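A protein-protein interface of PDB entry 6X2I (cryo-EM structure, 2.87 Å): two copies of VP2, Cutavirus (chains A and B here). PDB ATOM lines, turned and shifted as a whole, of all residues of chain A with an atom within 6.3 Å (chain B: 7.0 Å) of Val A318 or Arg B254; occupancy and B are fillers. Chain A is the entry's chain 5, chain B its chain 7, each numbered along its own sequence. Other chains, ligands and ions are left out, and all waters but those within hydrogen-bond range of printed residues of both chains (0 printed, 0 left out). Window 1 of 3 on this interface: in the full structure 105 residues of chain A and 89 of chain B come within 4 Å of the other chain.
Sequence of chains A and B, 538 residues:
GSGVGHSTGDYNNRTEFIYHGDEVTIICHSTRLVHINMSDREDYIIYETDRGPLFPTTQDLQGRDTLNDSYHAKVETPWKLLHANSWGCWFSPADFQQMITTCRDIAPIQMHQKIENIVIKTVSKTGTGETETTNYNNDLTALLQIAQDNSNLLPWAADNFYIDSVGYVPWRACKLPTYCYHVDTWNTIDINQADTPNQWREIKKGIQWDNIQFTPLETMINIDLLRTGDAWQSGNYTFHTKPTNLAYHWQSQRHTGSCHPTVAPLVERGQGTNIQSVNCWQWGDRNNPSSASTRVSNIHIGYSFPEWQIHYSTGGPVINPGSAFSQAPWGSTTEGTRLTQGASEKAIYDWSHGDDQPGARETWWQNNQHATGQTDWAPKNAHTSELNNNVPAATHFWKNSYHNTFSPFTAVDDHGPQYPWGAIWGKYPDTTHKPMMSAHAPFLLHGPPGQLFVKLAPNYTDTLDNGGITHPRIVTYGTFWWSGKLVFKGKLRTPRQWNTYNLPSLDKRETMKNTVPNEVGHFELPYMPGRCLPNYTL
The guanidinium group (NH1) of Arg B254 is in salt-bridge range of the side-chain carboxylate (OD2) of Asp A69 (2.5 Å). The backbone carbonyl oxygen (O) of Asp A69 sits close to the backbone NH (N) of Ser B293. The guanidinium group of Arg B254 sits close to the backbone carbonyl oxygen of Ser A70 (3.2 Å). The backbone NH (N) of Ile A310 sits at hydrogen-bond distance from the backbone carbonyl oxygen (O) of Ala B382, 2.5 Å away. A ring nitrogen (ND1) of His A311 sits at hydrogen-bond distance from the side-chain amide nitrogen (ND2) of Asn B381 (3.2 Å). The side-chain amide nitrogen (ND2) of Asn B381 lies close to the backbone NH (N) of Tyr A312, at 2.9 Å. N of Gly A315 sits at hydrogen-bond distance from OG of Ser B252. OG of Ser B293 sits at hydrogen-bond distance from O of Pro A317, at 2.9 Å. The backbone carbonyl oxygen of Tyr A71 sits close to the guanidinium group of Arg B254 (2.4 Å).
The backbone NH of Ser A70 sits at hydrogen-bond distance from the backbone carbonyl oxygen of Arg A51. The backbone NH (N) of Tyr A71 is in hydrogen-bond range of the backbone carbonyl oxygen (O) of Arg A51 (3.1 Å). OD2 of Asp A69 is in hydrogen-bond range of ND2 of Asn A187, 2.6 Å away. O of Gln A309 is in hydrogen-bond range of N of Asn A320. N of Val A318 lies within hydrogen-bond range of O of His A311 (2.6 Å). OG of Ser B252 lies close to N of Arg B254, at 3.4 Å.
NE2 of His A182 touches O of Thr B256, 3.8 Å away. CD2 of His A182 touches O of Gly B257 (3.6 Å). Ala B382 touches Gln A309 (O to NE2, 3.5 Å). His A311 touches His B300. Ser B252 touches Ser A313. Arg B254 touches Gly A315 (CZ to O, 3.8 Å). Gly A316 touches Arg B254 (CA to NH1, 3.5 Å). CA of Val A318 touches O of Ser B293, at 3.7 Å. Ser B293 touches Ile A319. Ile A319 touches Thr B294.
Of the printed residues of chain B, Asp A69 touches Arg B254 and Ser B293. Of the printed residues of chain B, His A182 touches Arg B254, His B255, Thr B256, Gly B257 and Cys B259. Printed residues of chain B within 4 Å of Gly A316: Arg B254. Val A318 touches just these residues of chain B: Arg B254, Ser B293 and His B300. Gln B251 touches none of the printed residues of chain A. Arg B254 touches eight residues of chain A. Of the printed residues of chain A, Cys B259 touches His A72 and His A182. Of the printed residues of chain A, Ala B292 touches Ser A70 (3.8 Å). The nearest residue of chain A that does not touch Arg B254 is Asn A187 (4.1 Å).
Of the 18 printed residues of chain B, 13 touch a printed residue of chain A. Hydrophobic or aromatic side chains of chain A that line the printed part of chain B: His A72, His A182, Ile A310, His A311, Pro A317, Val A318 and Ile A319.
No position is printed for both chains. Of the 33 pairs that touch across the chains among the printed residues, none has its exchanged pair printed and touching as well.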
ATOM      1  N   ARG A  51       8.368  34.506 -16.921  1.00  0.00           N
ATOM      2  CA  ARG A  51       7.378  34.399 -17.989  1.00  0.00           C
ATOM      3  C   ARG A  51       7.948  33.710 -19.218  1.00  0.00           C
ATOM      4  O   ARG A  51       7.531  32.607 -19.574  1.00  0.00           O
ATOM      5  CB  ARG A  51       6.869  35.780 -18.389  1.00  0.00           C
ATOM      6  CG  ARG A  51       6.021  36.472 -17.369  1.00  0.00           C
ATOM      7  CD  ARG A  51       4.717  35.753 -17.234  1.00  0.00           C
ATOM      8  NE  ARG A  51       3.795  36.442 -16.348  1.00  0.00           N
ATOM      9  CZ  ARG A  51       2.656  35.920 -15.921  1.00  0.00           C
ATOM     10  NH1 ARG A  51       1.869  36.614 -15.119  1.00  0.00           N
ATOM     11  NH2 ARG A  51       2.311  34.701 -16.296  1.00  0.00           N
ATOM     12  N   ASP A  69       3.216  33.035 -22.733  1.00  0.00           N
ATOM     13  CA  ASP A  69       3.602  32.710 -21.367  1.00  0.00           C
ATOM     14  C   ASP A  69       4.131  31.287 -21.273  1.00  0.00           C
ATOM     15  O   ASP A  69       3.431  30.335 -21.623  1.00  0.00           O
ATOM     16  CB  ASP A  69       2.398  32.891 -20.452  1.00  0.00           C
ATOM     17  CG  ASP A  69       2.676  32.473 -19.039  1.00  0.00           C
ATOM     18  OD1 ASP A  69       3.483  33.139 -18.371  1.00  0.00           O
ATOM     19  OD2 ASP A  69       2.077  31.478 -18.589  1.00  0.00           O
ATOM     20  N   SER A  70       5.379  31.146 -20.838  1.00  0.00           N
ATOM     21  CA  SER A  70       5.944  29.868 -20.433  1.00  0.00           C
ATOM     22  C   SER A  70       6.053  29.696 -18.920  1.00  0.00           C
ATOM     23  O   SER A  70       6.613  28.693 -18.476  1.00  0.00           O
ATOM     24  CB  SER A  70       7.313  29.666 -21.081  1.00  0.00           C
ATOM     25  OG  SER A  70       8.226  30.651 -20.651  1.00  0.00           O
ATOM     26  N   TYR A  71       5.574  30.653 -18.124  1.00  0.00           N
ATOM     27  CA  TYR A  71       5.761  30.610 -16.677  1.00  0.00           C
ATOM     28  C   TYR A  71       5.271  29.304 -16.075  1.00  0.00           C
ATOM     29  O   TYR A  71       4.198  28.807 -16.421  1.00  0.00           O
ATOM     30  CB  TYR A  71       5.023  31.768 -16.008  1.00  0.00           C
ATOM     31  CG  TYR A  71       4.990  31.657 -14.504  1.00  0.00           C
ATOM     32  CD1 TYR A  71       6.076  32.025 -13.742  1.00  0.00           C
ATOM     33  CD2 TYR A  71       3.876  31.165 -13.849  1.00  0.00           C
ATOM     34  CE1 TYR A  71       6.056  31.915 -12.376  1.00  0.00           C
ATOM     35  CE2 TYR A  71       3.847  31.050 -12.482  1.00  0.00           C
ATOM     36  CZ  TYR A  71       4.939  31.428 -11.753  1.00  0.00           C
ATOM     37  OH  TYR A  71       4.915  31.318 -10.390  1.00  0.00           O
ATOM     38  N   HIS A  72       6.049  28.766 -15.143  1.00  0.00           N
ATOM     39  CA  HIS A  72       5.669  27.564 -14.414  1.00  0.00           C
ATOM     40  C   HIS A  72       6.625  27.408 -13.242  1.00  0.00           C
ATOM     41  O   HIS A  72       7.493  28.250 -13.011  1.00  0.00           O
ATOM     42  CB  HIS A  72       5.679  26.340 -15.323  1.00  0.00           C
ATOM     43  CG  HIS A  72       7.031  25.988 -15.850  1.00  0.00           C
ATOM     44  ND1 HIS A  72       7.894  25.155 -15.179  1.00  0.00           N
ATOM     45  CD2 HIS A  72       7.682  26.385 -16.966  1.00  0.00           C
ATOM     46  CE1 HIS A  72       9.010  25.033 -15.872  1.00  0.00           C
ATOM     47  NE2 HIS A  72       8.909  25.774 -16.958  1.00  0.00           N
ATOM     48  N   HIS A 182       6.498  19.345 -12.751  1.00  0.00           N
ATOM     49  CA  HIS A 182       5.785  20.520 -12.289  1.00  0.00           C
ATOM     50  C   HIS A 182       5.402  20.397 -10.825  1.00  0.00           C
ATOM     51  O   HIS A 182       5.267  19.306 -10.276  1.00  0.00           O
ATOM     52  CB  HIS A 182       4.518  20.724 -13.111  1.00  0.00           C
ATOM     53  CG  HIS A 182       4.767  21.001 -14.557  1.00  0.00           C
ATOM     54  ND1 HIS A 182       5.157  22.237 -15.017  1.00  0.00           N
ATOM     55  CD2 HIS A 182       4.702  20.198 -15.641  1.00  0.00           C
ATOM     56  CE1 HIS A 182       5.297  22.188 -16.327  1.00  0.00           C
ATOM     57  NE2 HIS A 182       5.034  20.960 -16.730  1.00  0.00           N
ATOM     58  N   ASN A 187      -1.472  30.312 -12.283  1.00  0.00           N
ATOM     59  CA  ASN A 187      -1.204  31.392 -13.219  1.00  0.00           C
ATOM     60  C   ASN A 187      -2.513  31.698 -13.927  1.00  0.00           C
ATOM     61  O   ASN A 187      -2.956  30.912 -14.767  1.00  0.00           O
ATOM     62  CB  ASN A 187      -0.114  30.977 -14.202  1.00  0.00           C
ATOM     63  CG  ASN A 187       0.327  32.092 -15.100  1.00  0.00           C
ATOM     64  OD1 ASN A 187       0.243  33.263 -14.748  1.00  0.00           O
ATOM     65  ND2 ASN A 187       0.829  31.732 -16.270  1.00  0.00           N
ATOM     66  N   GLN A 309      -8.227  27.482 -30.261  1.00  0.00           N
ATOM     67  CA  GLN A 309      -8.828  27.727 -28.957  1.00  0.00           C
ATOM     68  C   GLN A 309      -7.736  27.921 -27.920  1.00  0.00           C
ATOM     69  O   GLN A 309      -6.899  27.038 -27.716  1.00  0.00           O
ATOM     70  CB  GLN A 309      -9.745  26.567 -28.583  1.00  0.00           C
ATOM     71  CG  GLN A 309     -10.453  26.667 -27.247  1.00  0.00           C
ATOM     72  CD  GLN A 309     -11.349  27.866 -27.130  1.00  0.00           C
ATOM     73  OE1 GLN A 309     -12.164  28.137 -28.000  1.00  0.00           O
ATOM     74  NE2 GLN A 309     -11.242  28.562 -26.019  1.00  0.00           N
ATOM     75  N   ILE A 310      -7.738  29.076 -27.272  1.00  0.00           N
ATOM     76  CA  ILE A 310      -6.763  29.404 -26.247  1.00  0.00           C
ATOM     77  C   ILE A 310      -7.479  29.288 -24.918  1.00  0.00           C
ATOM     78  O   ILE A 310      -8.311  30.131 -24.569  1.00  0.00           O
ATOM     79  CB  ILE A 310      -6.187  30.809 -26.433  1.00  0.00           C
ATOM     80  CG1 ILE A 310      -5.582  30.960 -27.819  1.00  0.00           C
ATOM     81  CG2 ILE A 310      -5.109  31.054 -25.415  1.00  0.00           C
ATOM     82  CD1 ILE A 310      -5.352  32.376 -28.195  1.00  0.00           C
ATOM     83  N   HIS A 311      -7.152  28.247 -24.176  1.00  0.00           N
ATOM     84  CA  HIS A 311      -7.728  28.006 -22.867  1.00  0.00           C
ATOM     85  C   HIS A 311      -6.841  28.624 -21.803  1.00  0.00           C
ATOM     86  O   HIS A 311      -5.687  28.226 -21.651  1.00  0.00           O
ATOM     87  CB  HIS A 311      -7.912  26.505 -22.660  1.00  0.00           C
ATOM     88  CG  HIS A 311      -8.110  26.095 -21.239  1.00  0.00           C
ATOM     89  ND1 HIS A 311      -8.957  26.750 -20.377  1.00  0.00           N
ATOM     90  CD2 HIS A 311      -7.631  25.034 -20.555  1.00  0.00           C
ATOM     91  CE1 HIS A 311      -8.931  26.155 -19.200  1.00  0.00           C
ATOM     92  NE2 HIS A 311      -8.153  25.097 -19.290  1.00  0.00           N
ATOM     93  N   TYR A 312      -7.376  29.593 -21.074  1.00  0.00           N
ATOM     94  CA  TYR A 312      -6.653  30.182 -19.959  1.00  0.00           C
ATOM     95  C   TYR A 312      -6.998  29.374 -18.723  1.00  0.00           C
ATOM     96  O   TYR A 312      -8.099  29.487 -18.181  1.00  0.00           O
ATOM     97  CB  TYR A 312      -7.020  31.650 -19.793  1.00  0.00           C
ATOM     98  CG  TYR A 312      -6.379  32.550 -20.813  1.00  0.00           C
ATOM     99  CD1 TYR A 312      -5.195  33.206 -20.529  1.00  0.00           C
ATOM    100  CD2 TYR A 312      -6.928  32.706 -22.071  1.00  0.00           C
ATOM    101  CE1 TYR A 312      -4.597  34.016 -21.451  1.00  0.00           C
ATOM    102  CE2 TYR A 312      -6.331  33.510 -23.004  1.00  0.00           C
ATOM    103  CZ  TYR A 312      -5.164  34.161 -22.686  1.00  0.00           C
ATOM    104  OH  TYR A 312      -4.558  34.969 -23.613  1.00  0.00           O
ATOM    105  N   SER A 313      -6.046  28.584 -18.266  1.00  0.00           N
ATOM    106  CA  SER A 313      -6.247  27.625 -17.200  1.00  0.00           C
ATOM    107  C   SER A 313      -5.597  28.133 -15.928  1.00  0.00           C
ATOM    108  O   SER A 313      -5.068  29.243 -15.871  1.00  0.00           O
ATOM    109  CB  SER A 313      -5.704  26.258 -17.609  1.00  0.00           C
ATOM    110  OG  SER A 313      -4.348  26.323 -17.976  1.00  0.00           O
ATOM    111  N   GLY A 315      -2.947  26.967 -14.727  1.00  0.00           N
ATOM    112  CA  GLY A 315      -1.517  26.939 -14.935  1.00  0.00           C
ATOM    113  C   GLY A 315      -1.049  27.972 -15.934  1.00  0.00           C
ATOM    114  O   GLY A 315       0.118  28.365 -15.931  1.00  0.00           O
ATOM    115  N   GLY A 316      -1.952  28.403 -16.805  1.00  0.00           N
ATOM    116  CA  GLY A 316      -1.676  29.439 -17.764  1.00  0.00           C
ATOM    117  C   GLY A 316      -2.455  29.185 -19.031  1.00  0.00           C
ATOM    118  O   GLY A 316      -3.251  28.252 -19.102  1.00  0.00           O
ATOM    119  N   PRO A 317      -2.238  29.994 -20.063  1.00  0.00           N
ATOM    120  CA  PRO A 317      -2.931  29.750 -21.329  1.00  0.00           C
ATOM    121  C   PRO A 317      -2.386  28.526 -22.050  1.00  0.00           C
ATOM    122  O   PRO A 317      -1.176  28.298 -22.099  1.00  0.00           O
ATOM    123  CB  PRO A 317      -2.667  31.032 -22.121  1.00  0.00           C
ATOM    124  CG  PRO A 317      -1.413  31.550 -21.559  1.00  0.00           C
ATOM    125  CD  PRO A 317      -1.474  31.248 -20.101  1.00  0.00           C
ATOM    126  N   VAL A 318      -3.298  27.740 -22.621  1.00  0.00           N
ATOM    127  CA  VAL A 318      -2.967  26.577 -23.432  1.00  0.00           C
ATOM    128  C   VAL A 318      -3.759  26.622 -24.723  1.00  0.00           C
ATOM    129  O   VAL A 318      -4.679  27.416 -24.896  1.00  0.00           O
ATOM    130  CB  VAL A 318      -3.248  25.244 -22.725  1.00  0.00           C
ATOM    131  CG1 VAL A 318      -2.258  24.995 -21.711  1.00  0.00           C
ATOM    132  CG2 VAL A 318      -4.592  25.282 -22.074  1.00  0.00           C
ATOM    133  N   ILE A 319      -3.384  25.739 -25.633  1.00  0.00           N
ATOM    134  CA  ILE A 319      -4.150  25.467 -26.835  1.00  0.00           C
ATOM    135  C   ILE A 319      -5.006  24.238 -26.590  1.00  0.00           C
ATOM    136  O   ILE A 319      -4.513  23.218 -26.098  1.00  0.00           O
ATOM    137  CB  ILE A 319      -3.230  25.263 -28.046  1.00  0.00           C
ATOM    138  CG1 ILE A 319      -2.484  26.554 -28.366  1.00  0.00           C
ATOM    139  CG2 ILE A 319      -4.017  24.784 -29.226  1.00  0.00           C
ATOM    140  CD1 ILE A 319      -3.377  27.709 -28.720  1.00  0.00           C
ATOM    141  N   ASN A 320      -6.291  24.343 -26.917  1.00  0.00           N
ATOM    142  CA  ASN A 320      -7.186  23.203 -26.906  1.00  0.00           C
ATOM    143  C   ASN A 320      -7.328  22.727 -28.342  1.00  0.00           C
ATOM    144  O   ASN A 320      -7.893  23.455 -29.166  1.00  0.00           O
ATOM    145  CB  ASN A 320      -8.540  23.599 -26.326  1.00  0.00           C
ATOM    146  CG  ASN A 320      -9.411  22.411 -26.013  1.00  0.00           C
ATOM    147  OD1 ASN A 320      -9.204  21.321 -26.533  1.00  0.00           O
ATOM    148  ND2 ASN A 320     -10.387  22.612 -25.148  1.00  0.00           N
ATOM    149  N   GLN B 251      -3.612  19.301 -11.164  1.00  0.00           N
ATOM    150  CA  GLN B 251      -2.820  19.591 -12.349  1.00  0.00           C
ATOM    151  C   GLN B 251      -3.710  20.053 -13.484  1.00  0.00           C
ATOM    152  O   GLN B 251      -4.700  19.396 -13.815  1.00  0.00           O
ATOM    153  CB  GLN B 251      -2.028  18.371 -12.800  1.00  0.00           C
ATOM    154  CG  GLN B 251      -0.965  17.931 -11.854  1.00  0.00           C
ATOM    155  CD  GLN B 251      -0.140  16.822 -12.422  1.00  0.00           C
ATOM    156  OE1 GLN B 251      -0.571  16.129 -13.316  1.00  0.00           O
ATOM    157  NE2 GLN B 251       1.064  16.658 -11.917  1.00  0.00           N
ATOM    158  N   SER B 252      -3.350  21.175 -14.086  1.00  0.00           N
ATOM    159  CA  SER B 252      -4.027  21.657 -15.272  1.00  0.00           C
ATOM    160  C   SER B 252      -3.308  21.106 -16.496  1.00  0.00           C
ATOM    161  O   SER B 252      -2.468  20.212 -16.396  1.00  0.00           O
ATOM    162  CB  SER B 252      -4.088  23.177 -15.282  1.00  0.00           C
ATOM    163  OG  SER B 252      -2.804  23.742 -15.395  1.00  0.00           O
ATOM    164  N   GLN B 253      -3.641  21.622 -17.670  1.00  0.00           N
ATOM    165  CA  GLN B 253      -2.968  21.157 -18.870  1.00  0.00           C
ATOM    166  C   GLN B 253      -1.517  21.615 -18.923  1.00  0.00           C
ATOM    167  O   GLN B 253      -0.708  20.982 -19.605  1.00  0.00           O
ATOM    168  CB  GLN B 253      -3.745  21.624 -20.097  1.00  0.00           C
ATOM    169  CG  GLN B 253      -3.282  21.017 -21.396  1.00  0.00           C
ATOM    170  CD  GLN B 253      -3.311  19.517 -21.349  1.00  0.00           C
ATOM    171  OE1 GLN B 253      -4.298  18.924 -20.940  1.00  0.00           O
ATOM    172  NE2 GLN B 253      -2.241  18.889 -21.795  1.00  0.00           N
ATOM    173  N   ARG B 254      -1.163  22.683 -18.214  1.00  0.00           N
ATOM    174  CA  ARG B 254       0.223  23.115 -18.123  1.00  0.00           C
ATOM    175  C   ARG B 254       0.956  22.613 -16.893  1.00  0.00           C
ATOM    176  O   ARG B 254       2.102  23.006 -16.683  1.00  0.00           O
ATOM    177  CB  ARG B 254       0.328  24.636 -18.192  1.00  0.00           C
ATOM    178  CG  ARG B 254       0.251  25.132 -19.597  1.00  0.00           C
ATOM    179  CD  ARG B 254       0.430  26.602 -19.706  1.00  0.00           C
ATOM    180  NE  ARG B 254       1.737  26.967 -19.207  1.00  0.00           N
ATOM    181  CZ  ARG B 254       2.174  28.210 -19.106  1.00  0.00           C
ATOM    182  NH1 ARG B 254       1.419  29.222 -19.488  1.00  0.00           N
ATOM    183  NH2 ARG B 254       3.377  28.434 -18.621  1.00  0.00           N
ATOM    184  N   HIS B 255       0.330  21.793 -16.061  1.00  0.00           N
ATOM    185  CA  HIS B 255       1.034  21.121 -14.983  1.00  0.00           C
ATOM    186  C   HIS B 255       1.392  19.681 -15.305  1.00  0.00           C
ATOM    187  O   HIS B 255       1.925  18.988 -14.438  1.00  0.00           O
ATOM    188  CB  HIS B 255       0.217  21.168 -13.698  1.00  0.00           C
ATOM    189  CG  HIS B 255      -0.066  22.553 -13.218  1.00  0.00           C
ATOM    190  ND1 HIS B 255       0.928  23.424 -12.843  1.00  0.00           N
ATOM    191  CD2 HIS B 255      -1.231  23.204 -13.019  1.00  0.00           C
ATOM    192  CE1 HIS B 255       0.387  24.563 -12.459  1.00  0.00           C
ATOM    193  NE2 HIS B 255      -0.922  24.455 -12.552  1.00  0.00           N
ATOM    194  N   THR B 256       1.107  19.206 -16.509  1.00  0.00           N
ATOM    195  CA  THR B 256       1.353  17.819 -16.868  1.00  0.00           C
ATOM    196  C   THR B 256       2.440  17.734 -17.925  1.00  0.00           C
ATOM    197  O   THR B 256       2.692  18.681 -18.671  1.00  0.00           O
ATOM    198  CB  THR B 256       0.090  17.136 -17.403  1.00  0.00           C
ATOM    199  OG1 THR B 256      -0.356  17.809 -18.584  1.00  0.00           O
ATOM    200  CG2 THR B 256      -1.013  17.159 -16.371  1.00  0.00           C
ATOM    201  N   GLY B 257       3.084  16.580 -17.971  1.00  0.00           N
ATOM    202  CA  GLY B 257       4.074  16.305 -18.981  1.00  0.00           C
ATOM    203  C   GLY B 257       5.436  16.854 -18.624  1.00  0.00           C
ATOM    204  O   GLY B 257       5.697  17.325 -17.519  1.00  0.00           O
ATOM    205  N   CYS B 259       8.241  19.418 -18.397  1.00  0.00           N
ATOM    206  CA  CYS B 259       8.252  20.862 -18.258  1.00  0.00           C
ATOM    207  C   CYS B 259       9.315  21.493 -19.148  1.00  0.00           C
ATOM    208  O   CYS B 259      10.292  20.858 -19.546  1.00  0.00           O
ATOM    209  CB  CYS B 259       8.451  21.253 -16.797  1.00  0.00           C
ATOM    210  SG  CYS B 259       9.741  20.396 -15.956  1.00  0.00           S
ATOM    211  N   TRP B 283       2.337  23.684 -31.583  1.00  0.00           N
ATOM    212  CA  TRP B 283       1.131  23.710 -32.389  1.00  0.00           C
ATOM    213  C   TRP B 283       1.261  24.770 -33.474  1.00  0.00           C
ATOM    214  O   TRP B 283       1.974  25.759 -33.319  1.00  0.00           O
ATOM    215  CB  TRP B 283      -0.109  23.992 -31.542  1.00  0.00           C
ATOM    216  CG  TRP B 283      -0.512  22.899 -30.616  1.00  0.00           C
ATOM    217  CD1 TRP B 283      -0.431  22.904 -29.267  1.00  0.00           C
ATOM    218  CD2 TRP B 283      -1.021  21.617 -30.981  1.00  0.00           C
ATOM    219  NE1 TRP B 283      -0.892  21.722 -28.758  1.00  0.00           N
ATOM    220  CE2 TRP B 283      -1.255  20.910 -29.796  1.00  0.00           C
ATOM    221  CE3 TRP B 283      -1.314  21.004 -32.197  1.00  0.00           C
ATOM    222  CZ2 TRP B 283      -1.757  19.621 -29.786  1.00  0.00           C
ATOM    223  CZ3 TRP B 283      -1.812  19.728 -32.187  1.00  0.00           C
ATOM    224  CH2 TRP B 283      -2.031  19.049 -30.992  1.00  0.00           C
ATOM    225  N   SER B 291       7.121  27.953 -26.522  1.00  0.00           N
ATOM    226  CA  SER B 291       6.732  28.231 -25.156  1.00  0.00           C
ATOM    227  C   SER B 291       5.870  27.096 -24.637  1.00  0.00           C
ATOM    228  O   SER B 291       5.302  26.324 -25.407  1.00  0.00           O
ATOM    229  CB  SER B 291       5.980  29.558 -25.068  1.00  0.00           C
ATOM    230  OG  SER B 291       4.813  29.525 -25.858  1.00  0.00           O
ATOM    231  N   ALA B 292       5.793  26.989 -23.313  1.00  0.00           N
ATOM    232  CA  ALA B 292       4.985  25.937 -22.721  1.00  0.00           C
ATOM    233  C   ALA B 292       3.517  26.109 -23.050  1.00  0.00           C
ATOM    234  O   ALA B 292       2.766  25.132 -23.015  1.00  0.00           O
ATOM    235  CB  ALA B 292       5.184  25.911 -21.211  1.00  0.00           C
ATOM    236  N   SER B 293       3.098  27.329 -23.370  1.00  0.00           N
ATOM    237  CA  SER B 293       1.714  27.573 -23.741  1.00  0.00           C
ATOM    238  C   SER B 293       1.332  26.769 -24.971  1.00  0.00           C
ATOM    239  O   SER B 293       0.392  25.970 -24.941  1.00  0.00           O
ATOM    240  CB  SER B 293       1.506  29.059 -23.984  1.00  0.00           C
ATOM    241  OG  SER B 293       0.191  29.309 -24.424  1.00  0.00           O
ATOM    242  N   THR B 294       2.057  26.952 -26.061  1.00  0.00           N
ATOM    243  CA  THR B 294       1.839  26.161 -27.260  1.00  0.00           C
ATOM    244  C   THR B 294       2.894  25.075 -27.290  1.00  0.00           C
ATOM    245  O   THR B 294       4.057  25.338 -27.582  1.00  0.00           O
ATOM    246  CB  THR B 294       1.922  27.013 -28.519  1.00  0.00           C
ATOM    247  OG1 THR B 294       3.185  27.678 -28.557  1.00  0.00           O
ATOM    248  CG2 THR B 294       0.833  28.024 -28.539  1.00  0.00           C
ATOM    249  N   ARG B 295       2.485  23.860 -26.983  1.00  0.00           N
ATOM    250  CA  ARG B 295       3.256  22.684 -27.316  1.00  0.00           C
ATOM    251  C   ARG B 295       2.256  21.555 -27.399  1.00  0.00           C
ATOM    252  O   ARG B 295       1.205  21.603 -26.755  1.00  0.00           O
ATOM    253  CB  ARG B 295       4.344  22.362 -26.293  1.00  0.00           C
ATOM    254  CG  ARG B 295       3.820  21.910 -24.978  1.00  0.00           C
ATOM    255  CD  ARG B 295       4.905  21.288 -24.152  1.00  0.00           C
ATOM    256  NE  ARG B 295       4.350  20.692 -22.946  1.00  0.00           N
ATOM    257  CZ  ARG B 295       3.744  19.516 -22.943  1.00  0.00           C
ATOM    258  NH1 ARG B 295       3.252  18.995 -21.835  1.00  0.00           N
ATOM    259  NH2 ARG B 295       3.603  18.879 -24.079  1.00  0.00           N
ATOM    260  N   HIS B 300      -6.423  16.878 -23.406  1.00  0.00           N
ATOM    261  CA  HIS B 300      -6.684  18.175 -22.802  1.00  0.00           C
ATOM    262  C   HIS B 300      -7.504  17.976 -21.542  1.00  0.00           C
ATOM    263  O   HIS B 300      -8.418  17.155 -21.515  1.00  0.00           O
ATOM    264  CB  HIS B 300      -7.416  19.120 -23.732  1.00  0.00           C
ATOM    265  CG  HIS B 300      -7.447  20.526 -23.232  1.00  0.00           C
ATOM    266  ND1 HIS B 300      -6.315  21.302 -23.144  1.00  0.00           N
ATOM    267  CD2 HIS B 300      -8.457  21.282 -22.748  1.00  0.00           C
ATOM    268  CE1 HIS B 300      -6.630  22.484 -22.655  1.00  0.00           C
ATOM    269  NE2 HIS B 300      -7.924  22.497 -22.401  1.00  0.00           N
ATOM    270  N   ILE B 301      -7.183  18.729 -20.500  1.00  0.00           N
ATOM    271  CA  ILE B 301      -7.845  18.597 -19.210  1.00  0.00           C
ATOM    272  C   ILE B 301      -8.867  19.715 -19.078  1.00  0.00           C
ATOM    273  O   ILE B 301      -8.509  20.892 -18.975  1.00  0.00           O
ATOM    274  CB  ILE B 301      -6.839  18.617 -18.054  1.00  0.00           C
ATOM    275  CG1 ILE B 301      -6.017  17.337 -18.057  1.00  0.00           C
ATOM    276  CG2 ILE B 301      -7.548  18.774 -16.743  1.00  0.00           C
ATOM    277  CD1 ILE B 301      -4.898  17.338 -17.096  1.00  0.00           C
ATOM    278  N   ASN B 381     -11.501  32.373 -21.921  1.00  0.00           N
ATOM    279  CA  ASN B 381     -10.789  31.794 -23.047  1.00  0.00           C
ATOM    280  C   ASN B 381     -10.887  32.695 -24.269  1.00  0.00           C
ATOM    281  O   ASN B 381     -11.762  33.555 -24.368  1.00  0.00           O
ATOM    282  CB  ASN B 381     -11.344  30.425 -23.402  1.00  0.00           C
ATOM    283  CG  ASN B 381     -11.331  29.476 -22.247  1.00  0.00           C
ATOM    284  OD1 ASN B 381     -12.287  28.744 -22.042  1.00  0.00           O
ATOM    285  ND2 ASN B 381     -10.270  29.500 -21.463  1.00  0.00           N
ATOM    286  N   ALA B 382      -9.981  32.475 -25.218  1.00  0.00           N
ATOM    287  CA  ALA B 382      -9.998  33.186 -26.488  1.00  0.00           C
ATOM    288  C   ALA B 382      -9.651  32.219 -27.609  1.00  0.00           C
ATOM    289  O   ALA B 382      -9.207  31.097 -27.369  1.00  0.00           O
ATOM    290  CB  ALA B 382      -9.028  34.364 -26.478  1.00  0.00           C
